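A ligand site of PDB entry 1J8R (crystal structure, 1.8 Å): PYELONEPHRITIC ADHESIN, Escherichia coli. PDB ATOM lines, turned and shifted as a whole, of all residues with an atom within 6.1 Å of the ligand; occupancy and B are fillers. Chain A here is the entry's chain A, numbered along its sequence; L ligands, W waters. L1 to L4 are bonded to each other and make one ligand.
NZ of Lys 172 is in salt-bridge range of OE1 of Glu 91 (2.8 Å). OE2 of Glu 91 lies within hydrogen-bond range of OG of Ser 89 (2.6 Å). The side-chain carboxylate (OE1) of Glu 91 lies within hydrogen-bond range of the side-chain hydroxyl (OH) of Tyr 175 (2.6 Å). The guanidinium group (NH1) of Arg 170 is in salt-bridge range of the side-chain carboxylate (OD2) of Asp 108 (2.7 Å). The backbone NH (N) of Ser 89 is in hydrogen-bond range of the backbone carbonyl oxygen (O) of Leu 102 (2.9 Å).
Ser 89 touches the ligand. O of Leu 102 touches O5 of LG3 L3, 3.8 Å away. CA of Lys 103 touches O5 of LG3 L3 (3.5 Å). CE3 of Trp 107 touches C5 of LG2 L2, at 3.5 Å. Of the 18 residues printed, 9 come within 4 Å of the ligand.
An oxygen (O5) of LG2 L2 is in hydrogen-bond range of the side-chain carboxylate of Glu 59, at 2.6 Å. OE2 of Glu 91 lies within hydrogen-bond range of O3 of LG3 L3 (2.7 Å). The backbone NH (N) of Gly 104 is in hydrogen-bond range of an oxygen (O5) of LG3 L3 (2.7 Å). The backbone carbonyl oxygen of Gly 104 lies within hydrogen-bond range of an oxygen (O2) of LG2 L2 (2.8 Å). The side-chain amino group (NZ) of Lys 172 is in hydrogen-bond range of an oxygen (O3) of LG3 L3, at 2.9 Å. NH2 of Arg 170 is in hydrogen-bond range of O3 of LIG L1 (3.1 Å).
Water W6 bridges O1 of LG3 L3 and OE1 of Glu 59. Water W1 bridges O5 of LG3 L3 and NZ of Lys 103. Water W8 lies within hydrogen-bond range of NZ of Lys 172 (2.6 Å) and O2 of LG4 L4 (2.9 Å). Water W5 lies within hydrogen-bond range of O5 of LIG L1 (3.1 Å) and NE1 of Trp 107 (3.1 Å). Water W3 lies within hydrogen-bond range of O4 of LG4 L4 (3.3 Å), OH of Tyr 175 (3.4 Å) and N of Asn 92 (3.4 Å).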
ATOM      1  N   GLU A  59     -30.241  21.750   5.603  1.00  0.00           N
ATOM      2  CA  GLU A  59     -28.938  22.387   5.429  1.00  0.00           C
ATOM      3  C   GLU A  59     -27.985  21.190   5.379  1.00  0.00           C
ATOM      4  O   GLU A  59     -27.828  20.488   6.373  1.00  0.00           O
ATOM      5  CB  GLU A  59     -28.541  23.313   6.591  1.00  0.00           C
ATOM      6  CG  GLU A  59     -27.221  24.013   6.298  1.00  0.00           C
ATOM      7  CD  GLU A  59     -26.578  24.683   7.487  1.00  0.00           C
ATOM      8  OE1 GLU A  59     -25.765  25.617   7.285  1.00  0.00           O
ATOM      9  OE2 GLU A  59     -26.835  24.254   8.633  1.00  0.00           O
ATOM     10  N   TYR A  60     -27.386  20.928   4.217  1.00  0.00           N
ATOM     11  CA  TYR A  60     -26.458  19.791   4.066  1.00  0.00           C
ATOM     12  C   TYR A  60     -25.021  20.271   3.830  1.00  0.00           C
ATOM     13  O   TYR A  60     -24.784  21.157   3.005  1.00  0.00           O
ATOM     14  CB  TYR A  60     -26.870  18.897   2.892  1.00  0.00           C
ATOM     15  CG  TYR A  60     -28.216  18.180   3.019  1.00  0.00           C
ATOM     16  CD1 TYR A  60     -28.735  17.470   1.931  1.00  0.00           C
ATOM     17  CD2 TYR A  60     -28.948  18.185   4.213  1.00  0.00           C
ATOM     18  CE1 TYR A  60     -29.954  16.763   2.027  1.00  0.00           C
ATOM     19  CE2 TYR A  60     -30.163  17.486   4.330  1.00  0.00           C
ATOM     20  CZ  TYR A  60     -30.659  16.779   3.237  1.00  0.00           C
ATOM     21  OH  TYR A  60     -31.857  16.111   3.332  1.00  0.00           O
ATOM     22  N   ILE A  61     -24.076  19.684   4.541  1.00  0.00           N
ATOM     23  CA  ILE A  61     -22.661  20.037   4.409  1.00  0.00           C
ATOM     24  C   ILE A  61     -21.803  18.777   4.319  1.00  0.00           C
ATOM     25  O   ILE A  61     -21.831  17.927   5.212  1.00  0.00           O
ATOM     26  CB  ILE A  61     -22.162  20.907   5.604  1.00  0.00           C
ATOM     27  CG1 ILE A  61     -23.005  22.181   5.730  1.00  0.00           C
ATOM     28  CG2 ILE A  61     -20.671  21.240   5.423  1.00  0.00           C
ATOM     29  CD1 ILE A  61     -22.687  23.025   7.010  1.00  0.00           C
ATOM     30  N   SER A  89     -13.923  23.917   0.918  1.00  0.00           N
ATOM     31  CA  SER A  89     -13.568  24.975   1.857  1.00  0.00           C
ATOM     32  C   SER A  89     -12.643  24.366   2.892  1.00  0.00           C
ATOM     33  O   SER A  89     -13.074  23.566   3.717  1.00  0.00           O
ATOM     34  CB  SER A  89     -14.836  25.517   2.529  1.00  0.00           C
ATOM     35  OG  SER A  89     -14.506  26.384   3.605  1.00  0.00           O
ATOM     36  N   GLU A  90     -11.356  24.733   2.835  1.00  0.00           N
ATOM     37  CA  GLU A  90     -10.364  24.209   3.773  1.00  0.00           C
ATOM     38  C   GLU A  90     -10.391  25.104   5.020  1.00  0.00           C
ATOM     39  O   GLU A  90     -10.009  26.280   4.968  1.00  0.00           O
ATOM     40  CB  GLU A  90      -8.976  24.204   3.121  1.00  0.00           C
ATOM     41  CG  GLU A  90      -7.882  23.563   3.969  1.00  0.00           C
ATOM     42  CD  GLU A  90      -6.528  23.514   3.253  1.00  0.00           C
ATOM     43  OE1 GLU A  90      -5.505  23.323   3.930  1.00  0.00           O
ATOM     44  OE2 GLU A  90      -6.494  23.662   2.020  1.00  0.00           O
ATOM     45  N   GLU A  91     -10.822  24.538   6.142  1.00  0.00           N
ATOM     46  CA  GLU A  91     -10.985  25.312   7.372  1.00  0.00           C
ATOM     47  C   GLU A  91     -10.197  24.820   8.572  1.00  0.00           C
ATOM     48  O   GLU A  91      -9.537  23.788   8.519  1.00  0.00           O
ATOM     49  CB  GLU A  91     -12.479  25.338   7.726  1.00  0.00           C
ATOM     50  CG  GLU A  91     -13.393  25.375   6.485  1.00  0.00           C
ATOM     51  CD  GLU A  91     -14.869  25.617   6.801  1.00  0.00           C
ATOM     52  OE1 GLU A  91     -15.290  25.394   7.953  1.00  0.00           O
ATOM     53  OE2 GLU A  91     -15.622  26.029   5.877  1.00  0.00           O
ATOM     54  N   ASN A  92     -10.283  25.575   9.664  1.00  0.00           N
ATOM     55  CA  ASN A  92      -9.609  25.248  10.909  1.00  0.00           C
ATOM     56  C   ASN A  92      -8.167  24.868  10.596  1.00  0.00           C
ATOM     57  O   ASN A  92      -7.650  23.882  11.125  1.00  0.00           O
ATOM     58  CB  ASN A  92     -10.322  24.096  11.610  1.00  0.00           C
ATOM     59  CG  ASN A  92      -9.837  23.877  13.024  1.00  0.00           C
ATOM     60  OD1 ASN A  92      -9.753  22.750  13.500  1.00  0.00           O
ATOM     61  ND2 ASN A  92      -9.528  24.965  13.694  1.00  0.00           N
ATOM     62  N   LEU A 102     -14.813  21.267   3.923  1.00  0.00           N
ATOM     63  CA  LEU A 102     -16.275  21.272   3.970  1.00  0.00           C
ATOM     64  C   LEU A 102     -16.867  21.812   2.691  1.00  0.00           C
ATOM     65  O   LEU A 102     -16.253  22.644   2.004  1.00  0.00           O
ATOM     66  CB  LEU A 102     -16.779  22.154   5.121  1.00  0.00           C
ATOM     67  CG  LEU A 102     -16.624  21.699   6.575  1.00  0.00           C
ATOM     68  CD1 LEU A 102     -15.152  21.722   6.994  1.00  0.00           C
ATOM     69  CD2 LEU A 102     -17.476  22.627   7.468  1.00  0.00           C
ATOM     70  N   LYS A 103     -18.055  21.333   2.356  1.00  0.00           N
ATOM     71  CA  LYS A 103     -18.759  21.839   1.204  1.00  0.00           C
ATOM     72  C   LYS A 103     -20.249  21.897   1.534  1.00  0.00           C
ATOM     73  O   LYS A 103     -20.950  20.868   1.506  1.00  0.00           O
ATOM     74  CB  LYS A 103     -18.484  20.982  -0.042  1.00  0.00           C
ATOM     75  CG  LYS A 103     -19.190  21.496  -1.296  1.00  0.00           C
ATOM     76  CD  LYS A 103     -19.070  23.008  -1.501  1.00  0.00           C
ATOM     77  CE  LYS A 103     -17.656  23.485  -1.732  1.00  0.00           C
ATOM     78  NZ  LYS A 103     -17.659  24.895  -2.287  1.00  0.00           N
ATOM     79  N   GLY A 104     -20.689  23.096   1.912  1.00  0.00           N
ATOM     80  CA  GLY A 104     -22.077  23.344   2.264  1.00  0.00           C
ATOM     81  C   GLY A 104     -22.751  23.764   0.977  1.00  0.00           C
ATOM     82  O   GLY A 104     -22.553  24.897   0.525  1.00  0.00           O
ATOM     83  N   TYR A 105     -23.568  22.871   0.410  1.00  0.00           N
ATOM     84  CA  TYR A 105     -24.206  23.122  -0.878  1.00  0.00           C
ATOM     85  C   TYR A 105     -25.715  23.222  -0.825  1.00  0.00           C
ATOM     86  O   TYR A 105     -26.363  23.380  -1.863  1.00  0.00           O
ATOM     87  CB  TYR A 105     -23.852  21.995  -1.861  1.00  0.00           C
ATOM     88  CG  TYR A 105     -24.561  20.689  -1.547  1.00  0.00           C
ATOM     89  CD1 TYR A 105     -25.667  20.297  -2.271  1.00  0.00           C
ATOM     90  CD2 TYR A 105     -24.128  19.882  -0.505  1.00  0.00           C
ATOM     91  CE1 TYR A 105     -26.349  19.117  -1.964  1.00  0.00           C
ATOM     92  CE2 TYR A 105     -24.802  18.698  -0.177  1.00  0.00           C
ATOM     93  CZ  TYR A 105     -25.901  18.333  -0.914  1.00  0.00           C
ATOM     94  OH  TYR A 105     -26.579  17.186  -0.607  1.00  0.00           O
ATOM     95  N   LYS A 106     -26.297  23.114   0.359  1.00  0.00           N
ATOM     96  CA  LYS A 106     -27.743  23.202   0.445  1.00  0.00           C
ATOM     97  C   LYS A 106     -28.074  23.895   1.769  1.00  0.00           C
ATOM     98  O   LYS A 106     -27.527  23.531   2.800  1.00  0.00           O
ATOM     99  CB  LYS A 106     -28.354  21.790   0.403  1.00  0.00           C
ATOM    100  CG  LYS A 106     -29.876  21.761   0.465  1.00  0.00           C
ATOM    101  CD  LYS A 106     -30.450  20.340   0.450  1.00  0.00           C
ATOM    102  CE  LYS A 106     -30.036  19.567  -0.808  1.00  0.00           C
ATOM    103  NZ  LYS A 106     -30.444  20.264  -2.063  1.00  0.00           N
ATOM    104  N   TRP A 107     -28.933  24.895   1.721  1.00  0.00           N
ATOM    105  CA  TRP A 107     -29.315  25.590   2.953  1.00  0.00           C
ATOM    106  C   TRP A 107     -30.685  26.216   2.776  1.00  0.00           C
ATOM    107  O   TRP A 107     -31.125  26.435   1.646  1.00  0.00           O
ATOM    108  CB  TRP A 107     -28.256  26.645   3.324  1.00  0.00           C
ATOM    109  CG  TRP A 107     -28.024  27.709   2.298  1.00  0.00           C
ATOM    110  CD1 TRP A 107     -28.707  28.887   2.148  1.00  0.00           C
ATOM    111  CD2 TRP A 107     -27.088  27.653   1.201  1.00  0.00           C
ATOM    112  NE1 TRP A 107     -28.262  29.567   1.033  1.00  0.00           N
ATOM    113  CE2 TRP A 107     -27.267  28.836   0.435  1.00  0.00           C
ATOM    114  CE3 TRP A 107     -26.112  26.726   0.802  1.00  0.00           C
ATOM    115  CZ2 TRP A 107     -26.510  29.096  -0.717  1.00  0.00           C
ATOM    116  CZ3 TRP A 107     -25.357  26.993  -0.338  1.00  0.00           C
ATOM    117  CH2 TRP A 107     -25.562  28.179  -1.087  1.00  0.00           C
ATOM    118  N   ASP A 108     -31.372  26.457   3.893  1.00  0.00           N
ATOM    119  CA  ASP A 108     -32.715  27.062   3.854  1.00  0.00           C
ATOM    120  C   ASP A 108     -33.672  26.361   2.900  1.00  0.00           C
ATOM    121  O   ASP A 108     -34.608  26.980   2.400  1.00  0.00           O
ATOM    122  CB  ASP A 108     -32.617  28.545   3.433  1.00  0.00           C
ATOM    123  CG  ASP A 108     -31.843  29.382   4.427  1.00  0.00           C
ATOM    124  OD1 ASP A 108     -31.387  30.495   4.049  1.00  0.00           O
ATOM    125  OD2 ASP A 108     -31.689  28.954   5.583  1.00  0.00           O
ATOM    126  N   ALA A 169     -31.820  28.511   9.314  1.00  0.00           N
ATOM    127  CA  ALA A 169     -31.124  27.650  10.247  1.00  0.00           C
ATOM    128  C   ALA A 169     -29.705  27.309   9.812  1.00  0.00           C
ATOM    129  O   ALA A 169     -29.465  26.890   8.675  1.00  0.00           O
ATOM    130  CB  ALA A 169     -31.941  26.367  10.504  1.00  0.00           C
ATOM    131  N   ARG A 170     -28.764  27.464  10.736  1.00  0.00           N
ATOM    132  CA  ARG A 170     -27.377  27.184  10.457  1.00  0.00           C
ATOM    133  C   ARG A 170     -26.727  26.393  11.580  1.00  0.00           C
ATOM    134  O   ARG A 170     -26.904  26.700  12.755  1.00  0.00           O
ATOM    135  CB  ARG A 170     -26.591  28.499  10.251  1.00  0.00           C
ATOM    136  CG  ARG A 170     -27.091  29.393   9.117  1.00  0.00           C
ATOM    137  CD  ARG A 170     -26.672  28.871   7.743  1.00  0.00           C
ATOM    138  NE  ARG A 170     -27.173  29.748   6.691  1.00  0.00           N
ATOM    139  CZ  ARG A 170     -28.429  29.780   6.266  1.00  0.00           C
ATOM    140  NH1 ARG A 170     -29.323  28.952   6.810  1.00  0.00           N
ATOM    141  NH2 ARG A 170     -28.804  30.656   5.351  1.00  0.00           N
ATOM    142  N   LYS A 172     -22.941  23.895  12.187  1.00  0.00           N
ATOM    143  CA  LYS A 172     -21.759  23.220  11.666  1.00  0.00           C
ATOM    144  C   LYS A 172     -21.278  22.341  12.797  1.00  0.00           C
ATOM    145  O   LYS A 172     -21.174  22.808  13.939  1.00  0.00           O
ATOM    146  CB  LYS A 172     -20.658  24.212  11.292  1.00  0.00           C
ATOM    147  CG  LYS A 172     -21.058  25.203  10.222  1.00  0.00           C
ATOM    148  CD  LYS A 172     -19.936  26.180   9.900  1.00  0.00           C
ATOM    149  CE  LYS A 172     -18.680  25.491   9.343  1.00  0.00           C
ATOM    150  NZ  LYS A 172     -17.696  26.526   8.900  1.00  0.00           N
ATOM    151  N   TYR A 175     -15.403  21.543  14.935  1.00  0.00           N
ATOM    152  CA  TYR A 175     -14.196  20.871  14.458  1.00  0.00           C
ATOM    153  C   TYR A 175     -13.684  19.845  15.445  1.00  0.00           C
ATOM    154  O   TYR A 175     -13.237  18.773  15.050  1.00  0.00           O
ATOM    155  CB  TYR A 175     -13.088  21.872  14.177  1.00  0.00           C
ATOM    156  CG  TYR A 175     -13.470  22.916  13.179  1.00  0.00           C
ATOM    157  CD1 TYR A 175     -13.571  24.262  13.549  1.00  0.00           C
ATOM    158  CD2 TYR A 175     -13.745  22.577  11.857  1.00  0.00           C
ATOM    159  CE1 TYR A 175     -13.929  25.230  12.620  1.00  0.00           C
ATOM    160  CE2 TYR A 175     -14.098  23.532  10.929  1.00  0.00           C
ATOM    161  CZ  TYR A 175     -14.190  24.859  11.310  1.00  0.00           C
ATOM    162  OH  TYR A 175     -14.535  25.810  10.377  1.00  0.00           O
HETATM  163  C1  LIG L   1     -27.034  33.247   2.935  1.00  0.00           C
HETATM  164  C2  LIG L   1     -25.779  32.453   3.270  1.00  0.00           C
HETATM  165  C3  LIG L   1     -25.103  32.041   1.933  1.00  0.00           C
HETATM  166  C4  LIG L   1     -24.762  33.327   1.118  1.00  0.00           C
HETATM  167  C5  LIG L   1     -24.130  33.027  -0.222  1.00  0.00           C
HETATM  168  C6  LIG L   1     -26.654  34.481   2.081  1.00  0.00           C
HETATM  169  O1  LIG L   1     -27.775  35.210   1.733  1.00  0.00           O
HETATM  170  O2  LIG L   1     -27.657  33.684   4.138  1.00  0.00           O
HETATM  171  O3  LIG L   1     -26.125  31.290   4.027  1.00  0.00           O
HETATM  172  O4  LIG L   1     -23.866  31.356   2.198  1.00  0.00           O
HETATM  173  O5  LIG L   1     -25.976  34.091   0.863  1.00  0.00           O
HETATM  174  O6  LIG L   1     -25.089  32.563  -1.180  1.00  0.00           O
HETATM  175  C1  LG2 L   2     -23.722  29.933   2.048  1.00  0.00           C
HETATM  176  C2  LG2 L   2     -22.382  29.326   1.634  1.00  0.00           C
HETATM  177  C3  LG2 L   2     -22.466  27.818   1.585  1.00  0.00           C
HETATM  178  C4  LG2 L   2     -22.771  27.326   2.974  1.00  0.00           C
HETATM  179  C5  LG2 L   2     -24.179  27.949   3.432  1.00  0.00           C
HETATM  180  C6  LG2 L   2     -24.734  27.611   4.816  1.00  0.00           C
HETATM  181  O1  LG2 L   2     -22.065  29.860   0.338  1.00  0.00           O
HETATM  182  O2  LG2 L   2     -21.216  27.278   1.215  1.00  0.00           O
HETATM  183  O3  LG2 L   2     -22.333  27.566   4.297  1.00  0.00           O
HETATM  184  O4  LG2 L   2     -24.165  29.429   3.338  1.00  0.00           O
HETATM  185  O5  LG2 L   2     -25.087  26.239   4.881  1.00  0.00           O
HETATM  186  C1  LG3 L   3     -21.605  26.568   5.033  1.00  0.00           C
HETATM  187  C2  LG3 L   3     -21.013  27.215   6.290  1.00  0.00           C
HETATM  188  C3  LG3 L   3     -19.819  28.069   5.941  1.00  0.00           C
HETATM  189  C4  LG3 L   3     -18.698  27.194   5.232  1.00  0.00           C
HETATM  190  C5  LG3 L   3     -19.303  26.619   3.975  1.00  0.00           C
HETATM  191  C6  LG3 L   3     -18.335  25.678   3.167  1.00  0.00           C
HETATM  192  O1  LG3 L   3     -21.982  27.965   6.940  1.00  0.00           O
HETATM  193  O2  LG3 L   3     -19.310  28.642   7.165  1.00  0.00           O
HETATM  194  O3  LG3 L   3     -18.272  26.172   6.039  1.00  0.00           O
HETATM  195  O4  LG3 L   3     -20.588  25.887   4.316  1.00  0.00           O
HETATM  196  O5  LG3 L   3     -18.999  25.246   1.962  1.00  0.00           O
HETATM  197  C1  LG4 L   4     -18.397  29.740   7.121  1.00  0.00           C
HETATM  198  C2  LG4 L   4     -18.526  30.459   8.419  1.00  0.00           C
HETATM  199  C3  LG4 L   4     -17.594  31.641   8.488  1.00  0.00           C
HETATM  200  C4  LG4 L   4     -16.146  31.131   8.310  1.00  0.00           C
HETATM  201  C5  LG4 L   4     -16.048  30.385   6.891  1.00  0.00           C
HETATM  202  C6  LG4 L   4     -14.721  29.749   6.458  1.00  0.00           C
HETATM  203  C7  LG4 L   4     -20.769  30.250   9.418  1.00  0.00           C
HETATM  204  C8  LG4 L   4     -20.265  29.579  10.686  1.00  0.00           C
HETATM  205  N1  LG4 L   4     -19.900  30.901   8.615  1.00  0.00           N
HETATM  206  O1  LG4 L   4     -17.803  32.279   9.766  1.00  0.00           O
HETATM  207  O2  LG4 L   4     -15.822  30.307   9.423  1.00  0.00           O
HETATM  208  O3  LG4 L   4     -17.042  29.315   6.808  1.00  0.00           O
HETATM  209  O4  LG4 L   4     -14.264  28.945   7.520  1.00  0.00           O
HETATM  210  O5  LG4 L   4     -21.955  30.179   9.150  1.00  0.00           O
HETATM  211  O   HOH W   1     -17.754  26.795  -0.086  1.00  0.00           O
HETATM  212  O   HOH W   2     -22.808  30.299   5.727  1.00  0.00           O
HETATM  213  O   HOH W   3     -12.287  28.277  10.085  1.00  0.00           O
HETATM  214  O   HOH W   4     -30.012  33.991   1.331  1.00  0.00           O
HETATM  215  O   HOH W   5     -28.443  32.471   0.049  1.00  0.00           O
HETATM  216  O   HOH W   6     -23.674  26.758   8.675  1.00  0.00           O
HETATM  217  O   HOH W   7     -22.908  28.088  11.060  1.00  0.00           O
HETATM  218  O   HOH W   8     -17.264  28.235  10.780  1.00  0.00           O
HETATM  219  O   HOH W   9     -24.794  24.274   3.051  1.00  0.00           O
